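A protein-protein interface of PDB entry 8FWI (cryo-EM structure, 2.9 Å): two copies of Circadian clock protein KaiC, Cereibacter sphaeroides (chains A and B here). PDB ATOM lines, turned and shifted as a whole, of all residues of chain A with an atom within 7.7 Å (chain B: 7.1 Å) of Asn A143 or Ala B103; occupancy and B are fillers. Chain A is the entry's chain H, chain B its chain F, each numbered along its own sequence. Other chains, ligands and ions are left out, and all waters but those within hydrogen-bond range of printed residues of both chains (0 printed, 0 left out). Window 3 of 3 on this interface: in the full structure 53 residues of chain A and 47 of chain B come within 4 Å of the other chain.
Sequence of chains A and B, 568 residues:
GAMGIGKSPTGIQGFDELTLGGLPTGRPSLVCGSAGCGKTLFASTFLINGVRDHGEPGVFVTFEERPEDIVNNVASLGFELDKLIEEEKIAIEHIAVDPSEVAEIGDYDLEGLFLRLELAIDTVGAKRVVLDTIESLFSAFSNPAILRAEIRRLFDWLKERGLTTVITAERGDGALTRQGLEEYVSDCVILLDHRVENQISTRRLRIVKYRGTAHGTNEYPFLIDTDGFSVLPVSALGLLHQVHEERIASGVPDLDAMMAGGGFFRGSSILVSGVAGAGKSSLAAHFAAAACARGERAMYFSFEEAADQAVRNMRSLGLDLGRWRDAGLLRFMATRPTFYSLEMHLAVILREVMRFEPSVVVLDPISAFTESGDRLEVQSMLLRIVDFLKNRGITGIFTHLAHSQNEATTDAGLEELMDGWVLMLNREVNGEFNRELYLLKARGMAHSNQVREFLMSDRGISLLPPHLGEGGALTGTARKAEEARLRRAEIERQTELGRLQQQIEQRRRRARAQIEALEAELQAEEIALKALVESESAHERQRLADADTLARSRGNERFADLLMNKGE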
ATOM      1  N   ILE A 105      -8.412 -10.082 -20.345  1.00  0.00           N
ATOM      2  CA  ILE A 105      -8.093  -8.799 -19.724  1.00  0.00           C
ATOM      3  C   ILE A 105      -9.180  -7.780 -20.031  1.00  0.00           C
ATOM      4  O   ILE A 105      -9.751  -7.758 -21.131  1.00  0.00           O
ATOM      5  CB  ILE A 105      -6.729  -8.265 -20.209  1.00  0.00           C
ATOM      6  CG1 ILE A 105      -6.736  -8.024 -21.722  1.00  0.00           C
ATOM      7  CG2 ILE A 105      -5.598  -9.202 -19.844  1.00  0.00           C
ATOM      8  CD1 ILE A 105      -5.483  -7.339 -22.227  1.00  0.00           C
ATOM      9  N   ALA A 140      -7.579 -13.924 -14.925  1.00  0.00           N
ATOM     10  CA  ALA A 140      -7.782 -13.823 -16.364  1.00  0.00           C
ATOM     11  C   ALA A 140      -6.642 -13.066 -17.030  1.00  0.00           C
ATOM     12  O   ALA A 140      -6.092 -13.514 -18.041  1.00  0.00           O
ATOM     13  CB  ALA A 140      -9.119 -13.138 -16.639  1.00  0.00           C
ATOM     14  N   PHE A 141      -6.278 -11.909 -16.480  1.00  0.00           N
ATOM     15  CA  PHE A 141      -5.278 -11.064 -17.116  1.00  0.00           C
ATOM     16  C   PHE A 141      -3.975 -11.823 -17.327  1.00  0.00           C
ATOM     17  O   PHE A 141      -3.409 -12.376 -16.379  1.00  0.00           O
ATOM     18  CB  PHE A 141      -5.023  -9.806 -16.276  1.00  0.00           C
ATOM     19  CG  PHE A 141      -6.221  -8.904 -16.123  1.00  0.00           C
ATOM     20  CD1 PHE A 141      -7.151  -9.113 -15.120  1.00  0.00           C
ATOM     21  CD2 PHE A 141      -6.383  -7.808 -16.949  1.00  0.00           C
ATOM     22  CE1 PHE A 141      -8.239  -8.268 -14.979  1.00  0.00           C
ATOM     23  CE2 PHE A 141      -7.454  -6.976 -16.809  1.00  0.00           C
ATOM     24  CZ  PHE A 141      -8.385  -7.198 -15.824  1.00  0.00           C
ATOM     25  N   SER A 142      -3.496 -11.848 -18.574  1.00  0.00           N
ATOM     26  CA  SER A 142      -2.323 -12.635 -18.937  1.00  0.00           C
ATOM     27  C   SER A 142      -1.165 -11.806 -19.493  1.00  0.00           C
ATOM     28  O   SER A 142      -0.207 -12.390 -20.011  1.00  0.00           O
ATOM     29  CB  SER A 142      -2.714 -13.716 -19.946  1.00  0.00           C
ATOM     30  OG  SER A 142      -3.645 -14.620 -19.379  1.00  0.00           O
ATOM     31  N   ASN A 143      -1.218 -10.475 -19.406  1.00  0.00           N
ATOM     32  CA  ASN A 143      -0.047  -9.661 -19.713  1.00  0.00           C
ATOM     33  C   ASN A 143       0.432  -8.971 -18.445  1.00  0.00           C
ATOM     34  O   ASN A 143      -0.372  -8.304 -17.778  1.00  0.00           O
ATOM     35  CB  ASN A 143      -0.353  -8.613 -20.793  1.00  0.00           C
ATOM     36  CG  ASN A 143       0.850  -7.741 -21.119  1.00  0.00           C
ATOM     37  OD1 ASN A 143       0.767  -6.514 -21.091  1.00  0.00           O
ATOM     38  ND2 ASN A 143       1.974  -8.374 -21.441  1.00  0.00           N
ATOM     39  N   PRO A 144       1.710  -9.101 -18.071  1.00  0.00           N
ATOM     40  CA  PRO A 144       2.133  -8.583 -16.756  1.00  0.00           C
ATOM     41  C   PRO A 144       1.828  -7.110 -16.537  1.00  0.00           C
ATOM     42  O   PRO A 144       1.428  -6.725 -15.432  1.00  0.00           O
ATOM     43  CB  PRO A 144       3.642  -8.857 -16.759  1.00  0.00           C
ATOM     44  CG  PRO A 144       3.795 -10.043 -17.632  1.00  0.00           C
ATOM     45  CD  PRO A 144       2.802  -9.834 -18.736  1.00  0.00           C
ATOM     46  N   ALA A 145       2.007  -6.271 -17.560  1.00  0.00           N
ATOM     47  CA  ALA A 145       1.803  -4.836 -17.383  1.00  0.00           C
ATOM     48  C   ALA A 145       0.330  -4.497 -17.188  1.00  0.00           C
ATOM     49  O   ALA A 145      -0.026  -3.722 -16.289  1.00  0.00           O
ATOM     50  CB  ALA A 145       2.367  -4.085 -18.589  1.00  0.00           C
ATOM     51  N   ILE A 146      -0.540  -5.075 -18.017  1.00  0.00           N
ATOM     52  CA  ILE A 146      -1.964  -4.764 -17.949  1.00  0.00           C
ATOM     53  C   ILE A 146      -2.527  -5.170 -16.591  1.00  0.00           C
ATOM     54  O   ILE A 146      -3.337  -4.448 -15.988  1.00  0.00           O
ATOM     55  CB  ILE A 146      -2.692  -5.463 -19.114  1.00  0.00           C
ATOM     56  CG1 ILE A 146      -2.071  -5.036 -20.450  1.00  0.00           C
ATOM     57  CG2 ILE A 146      -4.181  -5.150 -19.094  1.00  0.00           C
ATOM     58  CD1 ILE A 146      -2.874  -5.422 -21.671  1.00  0.00           C
ATOM     59  N   LEU A 147      -2.098  -6.327 -16.087  1.00  0.00           N
ATOM     60  CA  LEU A 147      -2.561  -6.793 -14.786  1.00  0.00           C
ATOM     61  C   LEU A 147      -2.136  -5.846 -13.674  1.00  0.00           C
ATOM     62  O   LEU A 147      -2.929  -5.534 -12.777  1.00  0.00           O
ATOM     63  CB  LEU A 147      -2.019  -8.196 -14.524  1.00  0.00           C
ATOM     64  CG  LEU A 147      -2.209  -8.751 -13.115  1.00  0.00           C
ATOM     65  CD1 LEU A 147      -3.668  -9.010 -12.819  1.00  0.00           C
ATOM     66  CD2 LEU A 147      -1.405 -10.020 -12.983  1.00  0.00           C
ATOM     67  N   ARG A 148      -0.881  -5.395 -13.698  1.00  0.00           N
ATOM     68  CA  ARG A 148      -0.423  -4.473 -12.669  1.00  0.00           C
ATOM     69  C   ARG A 148      -1.190  -3.163 -12.741  1.00  0.00           C
ATOM     70  O   ARG A 148      -1.525  -2.583 -11.701  1.00  0.00           O
ATOM     71  CB  ARG A 148       1.082  -4.234 -12.809  1.00  0.00           C
ATOM     72  CG  ARG A 148       1.661  -3.198 -11.852  1.00  0.00           C
ATOM     73  CD  ARG A 148       3.088  -2.835 -12.224  1.00  0.00           C
ATOM     74  NE  ARG A 148       4.061  -3.685 -11.549  1.00  0.00           N
ATOM     75  CZ  ARG A 148       4.558  -3.450 -10.341  1.00  0.00           C
ATOM     76  NH1 ARG A 148       4.198  -2.389  -9.639  1.00  0.00           N
ATOM     77  NH2 ARG A 148       5.437  -4.302  -9.826  1.00  0.00           N
ATOM     78  N   ALA A 149      -1.518  -2.708 -13.952  1.00  0.00           N
ATOM     79  CA  ALA A 149      -2.299  -1.483 -14.080  1.00  0.00           C
ATOM     80  C   ALA A 149      -3.685  -1.649 -13.474  1.00  0.00           C
ATOM     81  O   ALA A 149      -4.168  -0.763 -12.761  1.00  0.00           O
ATOM     82  CB  ALA A 149      -2.402  -1.081 -15.549  1.00  0.00           C
ATOM     83  N   GLN A 179       0.581 -14.697  -8.740  1.00  0.00           N
ATOM     84  CA  GLN A 179       0.957 -13.907  -9.904  1.00  0.00           C
ATOM     85  C   GLN A 179       2.110 -12.951  -9.630  1.00  0.00           C
ATOM     86  O   GLN A 179       2.690 -12.416 -10.581  1.00  0.00           O
ATOM     87  CB  GLN A 179      -0.262 -13.138 -10.422  1.00  0.00           C
ATOM     88  CG  GLN A 179      -1.202 -14.009 -11.243  1.00  0.00           C
ATOM     89  CD  GLN A 179      -2.542 -13.354 -11.503  1.00  0.00           C
ATOM     90  OE1 GLN A 179      -3.284 -13.041 -10.572  1.00  0.00           O
ATOM     91  NE2 GLN A 179      -2.870 -13.165 -12.776  1.00  0.00           N
ATOM     92  N   LEU A 181       2.575  -9.890  -8.117  1.00  0.00           N
ATOM     93  CA  LEU A 181       2.534  -8.443  -8.293  1.00  0.00           C
ATOM     94  C   LEU A 181       1.803  -7.691  -7.191  1.00  0.00           C
ATOM     95  O   LEU A 181       2.101  -6.516  -6.974  1.00  0.00           O
ATOM     96  CB  LEU A 181       1.877  -8.094  -9.634  1.00  0.00           C
ATOM     97  CG  LEU A 181       2.584  -8.647 -10.871  1.00  0.00           C
ATOM     98  CD1 LEU A 181       1.583  -8.806 -11.981  1.00  0.00           C
ATOM     99  CD2 LEU A 181       3.724  -7.750 -11.311  1.00  0.00           C
ATOM    100  N   ASP B  98      -1.957   4.595 -17.794  1.00  0.00           N
ATOM    101  CA  ASP B  98      -3.217   3.867 -17.856  1.00  0.00           C
ATOM    102  C   ASP B  98      -3.006   2.473 -18.437  1.00  0.00           C
ATOM    103  O   ASP B  98      -1.960   2.187 -19.025  1.00  0.00           O
ATOM    104  CB  ASP B  98      -4.231   4.630 -18.700  1.00  0.00           C
ATOM    105  CG  ASP B  98      -5.172   5.509 -17.888  1.00  0.00           C
ATOM    106  OD1 ASP B  98      -5.093   5.490 -16.642  1.00  0.00           O
ATOM    107  OD2 ASP B  98      -5.983   6.234 -18.504  1.00  0.00           O
ATOM    108  N   PRO B  99      -3.986   1.576 -18.279  1.00  0.00           N
ATOM    109  CA  PRO B  99      -3.804   0.215 -18.814  1.00  0.00           C
ATOM    110  C   PRO B  99      -3.481   0.170 -20.299  1.00  0.00           C
ATOM    111  O   PRO B  99      -2.589  -0.585 -20.708  1.00  0.00           O
ATOM    112  CB  PRO B  99      -5.151  -0.449 -18.509  1.00  0.00           C
ATOM    113  CG  PRO B  99      -5.624   0.242 -17.286  1.00  0.00           C
ATOM    114  CD  PRO B  99      -5.233   1.683 -17.497  1.00  0.00           C
ATOM    115  N   SER B 100      -4.177   0.957 -21.124  1.00  0.00           N
ATOM    116  CA  SER B 100      -3.886   0.955 -22.555  1.00  0.00           C
ATOM    117  C   SER B 100      -2.491   1.500 -22.831  1.00  0.00           C
ATOM    118  O   SER B 100      -1.810   1.050 -23.761  1.00  0.00           O
ATOM    119  CB  SER B 100      -4.934   1.776 -23.307  1.00  0.00           C
ATOM    120  OG  SER B 100      -4.954   3.116 -22.850  1.00  0.00           O
ATOM    121  N   GLU B 101      -2.052   2.471 -22.031  1.00  0.00           N
ATOM    122  CA  GLU B 101      -0.753   3.095 -22.254  1.00  0.00           C
ATOM    123  C   GLU B 101       0.373   2.070 -22.215  1.00  0.00           C
ATOM    124  O   GLU B 101       1.311   2.131 -23.019  1.00  0.00           O
ATOM    125  CB  GLU B 101      -0.517   4.170 -21.195  1.00  0.00           C
ATOM    126  CG  GLU B 101       0.791   4.924 -21.350  1.00  0.00           C
ATOM    127  CD  GLU B 101       0.838   5.744 -22.625  1.00  0.00           C
ATOM    128  OE1 GLU B 101      -0.239   6.127 -23.127  1.00  0.00           O
ATOM    129  OE2 GLU B 101       1.951   6.003 -23.131  1.00  0.00           O
ATOM    130  N   VAL B 102       0.294   1.116 -21.289  1.00  0.00           N
ATOM    131  CA  VAL B 102       1.411   0.236 -20.967  1.00  0.00           C
ATOM    132  C   VAL B 102       1.317  -1.099 -21.694  1.00  0.00           C
ATOM    133  O   VAL B 102       1.962  -2.069 -21.286  1.00  0.00           O
ATOM    134  CB  VAL B 102       1.500   0.020 -19.449  1.00  0.00           C
ATOM    135  CG1 VAL B 102       1.743   1.336 -18.756  1.00  0.00           C
ATOM    136  CG2 VAL B 102       0.220  -0.624 -18.922  1.00  0.00           C
ATOM    137  N   ALA B 103       0.525  -1.175 -22.761  1.00  0.00           N
ATOM    138  CA  ALA B 103       0.226  -2.468 -23.363  1.00  0.00           C
ATOM    139  C   ALA B 103       1.475  -3.169 -23.899  1.00  0.00           C
ATOM    140  O   ALA B 103       1.661  -4.367 -23.656  1.00  0.00           O
ATOM    141  CB  ALA B 103      -0.823  -2.297 -24.462  1.00  0.00           C
ATOM    142  N   GLU B 104       2.349  -2.458 -24.620  1.00  0.00           N
ATOM    143  CA  GLU B 104       3.366  -3.174 -25.395  1.00  0.00           C
ATOM    144  C   GLU B 104       4.689  -2.403 -25.396  1.00  0.00           C
ATOM    145  O   GLU B 104       4.857  -1.407 -24.685  1.00  0.00           O
ATOM    146  CB  GLU B 104       2.876  -3.392 -26.830  1.00  0.00           C
ATOM    147  CG  GLU B 104       2.046  -4.632 -27.033  1.00  0.00           C
ATOM    148  CD  GLU B 104       1.609  -4.917 -28.459  1.00  0.00           C
ATOM    149  OE1 GLU B 104       1.714  -4.017 -29.320  1.00  0.00           O
ATOM    150  OE2 GLU B 104       1.157  -6.056 -28.717  1.00  0.00           O
ATOM    151  N   ILE B 105       5.631  -2.891 -26.221  1.00  0.00           N
ATOM    152  CA  ILE B 105       6.933  -2.254 -26.404  1.00  0.00           C
ATOM    153  C   ILE B 105       6.778  -0.945 -27.164  1.00  0.00           C
ATOM    154  O   ILE B 105       5.948  -0.825 -28.075  1.00  0.00           O
ATOM    155  CB  ILE B 105       7.908  -3.181 -27.160  1.00  0.00           C
ATOM    156  CG1 ILE B 105       7.386  -3.510 -28.562  1.00  0.00           C
ATOM    157  CG2 ILE B 105       8.169  -4.462 -26.397  1.00  0.00           C
ATOM    158  CD1 ILE B 105       8.382  -4.273 -29.409  1.00  0.00           C
ATOM    159  N   ASP B 107       5.384   1.594 -26.643  1.00  0.00           N
ATOM    160  CA  ASP B 107       4.097   2.261 -26.531  1.00  0.00           C
ATOM    161  C   ASP B 107       4.260   3.635 -25.907  1.00  0.00           C
ATOM    162  O   ASP B 107       3.642   4.611 -26.348  1.00  0.00           O
ATOM    163  CB  ASP B 107       3.149   1.397 -25.703  1.00  0.00           C
ATOM    164  CG  ASP B 107       2.466   0.327 -26.528  1.00  0.00           C
ATOM    165  OD1 ASP B 107       3.033  -0.081 -27.563  1.00  0.00           O
ATOM    166  OD2 ASP B 107       1.363  -0.110 -26.137  1.00  0.00           O
ATOM    167  N   TYR B 108       5.101   3.732 -24.885  1.00  0.00           N
ATOM    168  CA  TYR B 108       5.370   5.004 -24.247  1.00  0.00           C
ATOM    169  C   TYR B 108       6.408   5.772 -25.053  1.00  0.00           C
ATOM    170  O   TYR B 108       7.438   5.222 -25.453  1.00  0.00           O
ATOM    171  CB  TYR B 108       5.869   4.781 -22.822  1.00  0.00           C
ATOM    172  CG  TYR B 108       5.643   5.970 -21.937  1.00  0.00           C
ATOM    173  CD1 TYR B 108       4.367   6.275 -21.481  1.00  0.00           C
ATOM    174  CD2 TYR B 108       6.687   6.794 -21.568  1.00  0.00           C
ATOM    175  CE1 TYR B 108       4.135   7.376 -20.674  1.00  0.00           C
ATOM    176  CE2 TYR B 108       6.470   7.884 -20.765  1.00  0.00           C
ATOM    177  CZ  TYR B 108       5.205   8.177 -20.314  1.00  0.00           C
ATOM    178  OH  TYR B 108       5.015   9.276 -19.510  1.00  0.00           O
ATOM    179  N   SER B 139       7.761  -3.275 -17.633  1.00  0.00           N
ATOM    180  CA  SER B 139       7.252  -4.643 -17.603  1.00  0.00           C
ATOM    181  C   SER B 139       6.521  -4.983 -18.888  1.00  0.00           C
ATOM    182  O   SER B 139       6.351  -6.165 -19.204  1.00  0.00           O
ATOM    183  CB  SER B 139       6.315  -4.855 -16.414  1.00  0.00           C
ATOM    184  OG  SER B 139       5.341  -3.832 -16.335  1.00  0.00           O
ATOM    185  N   ALA B 140       6.084  -3.965 -19.628  1.00  0.00           N
ATOM    186  CA  ALA B 140       5.382  -4.192 -20.883  1.00  0.00           C
ATOM    187  C   ALA B 140       6.283  -4.877 -21.902  1.00  0.00           C
ATOM    188  O   ALA B 140       5.885  -5.861 -22.535  1.00  0.00           O
ATOM    189  CB  ALA B 140       4.872  -2.858 -21.424  1.00  0.00           C
ATOM    190  N   PHE B 141       7.500  -4.367 -22.078  1.00  0.00           N
ATOM    191  CA  PHE B 141       8.383  -4.886 -23.112  1.00  0.00           C
ATOM    192  C   PHE B 141       8.609  -6.382 -22.937  1.00  0.00           C
ATOM    193  O   PHE B 141       9.026  -6.834 -21.866  1.00  0.00           O
ATOM    194  CB  PHE B 141       9.725  -4.145 -23.094  1.00  0.00           C
ATOM    195  CG  PHE B 141       9.631  -2.672 -23.399  1.00  0.00           C
ATOM    196  CD1 PHE B 141       9.365  -1.751 -22.402  1.00  0.00           C
ATOM    197  CD2 PHE B 141       9.871  -2.205 -24.677  1.00  0.00           C
ATOM    198  CE1 PHE B 141       9.297  -0.398 -22.690  1.00  0.00           C
ATOM    199  CE2 PHE B 141       9.803  -0.873 -24.961  1.00  0.00           C
ATOM    200  CZ  PHE B 141       9.520   0.037 -23.971  1.00  0.00           C
ATOM    201  N   SER B 142       8.334  -7.152 -23.994  1.00  0.00           N
ATOM    202  CA  SER B 142       8.395  -8.608 -23.927  1.00  0.00           C
ATOM    203  C   SER B 142       9.401  -9.235 -24.890  1.00  0.00           C
ATOM    204  O   SER B 142       9.389 -10.460 -25.056  1.00  0.00           O
ATOM    205  CB  SER B 142       7.007  -9.197 -24.176  1.00  0.00           C
ATOM    206  OG  SER B 142       6.095  -8.785 -23.172  1.00  0.00           O
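The side-chain hydroxyl (OG) of Ser B142 sits at hydrogen-bond distance from the backbone carbonyl oxygen (O) of Ala B140 (3.0 Å).
4 positions are printed for both chains.
Of the 5 pairs that touch across the chains among the printed residues, none has its exchanged pair printed and touching as well.
CB of Ala A145 touches O of Val B102 (3.4 Å).
CB of Ala A145 touches OG of Ser B139, at 3.7 Å.
Ala A145 touches Ala B140.
Pro B99 touches Ala A149.
The side-chain amide oxygen (OD1) of Asn A143 lies close to the backbone carbonyl oxygen (O) of Ala B103 (3.5 Å).
Hydrophobic or aromatic side chains of chain A that line the printed part of chain B: Ala A145 and Ala A149.
Hydrophobic or aromatic side chains of chain B that line the printed part of chain A: Pro B99 and Ala B140.
Among the printed residues, 5 pairs touch across the chains.
Among the printed residues, no Asp or Glu carboxylate lies within 4 Å of a Lys or Arg side-chain nitrogen of the other chain.
Ala A140 touches none of the printed residues of chain B.
Asn A143 touches just one residue of chain B: Ala B103 (3.5 Å).
Of the printed residues of chain B, Ala A145 touches Val B102 (3.4 Å), Ser B139 (3.7 Å) and Ala B140 (3.8 Å).
Arg A148 touches none of the printed residues of chain B.
Printed residues of chain B within 4 Å of Ala A149: Pro B99.
Of the printed residues of chain A, Pro B99 touches Ala A149 (3.8 Å).
Ala B103 touches just one residue of chain A: Asn A143 (3.5 Å).
Printed residues of chain A within 4 Å of Ser B139: Ala A145.
Of the printed residues of chain A, Ala B140 touches Ala A145.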
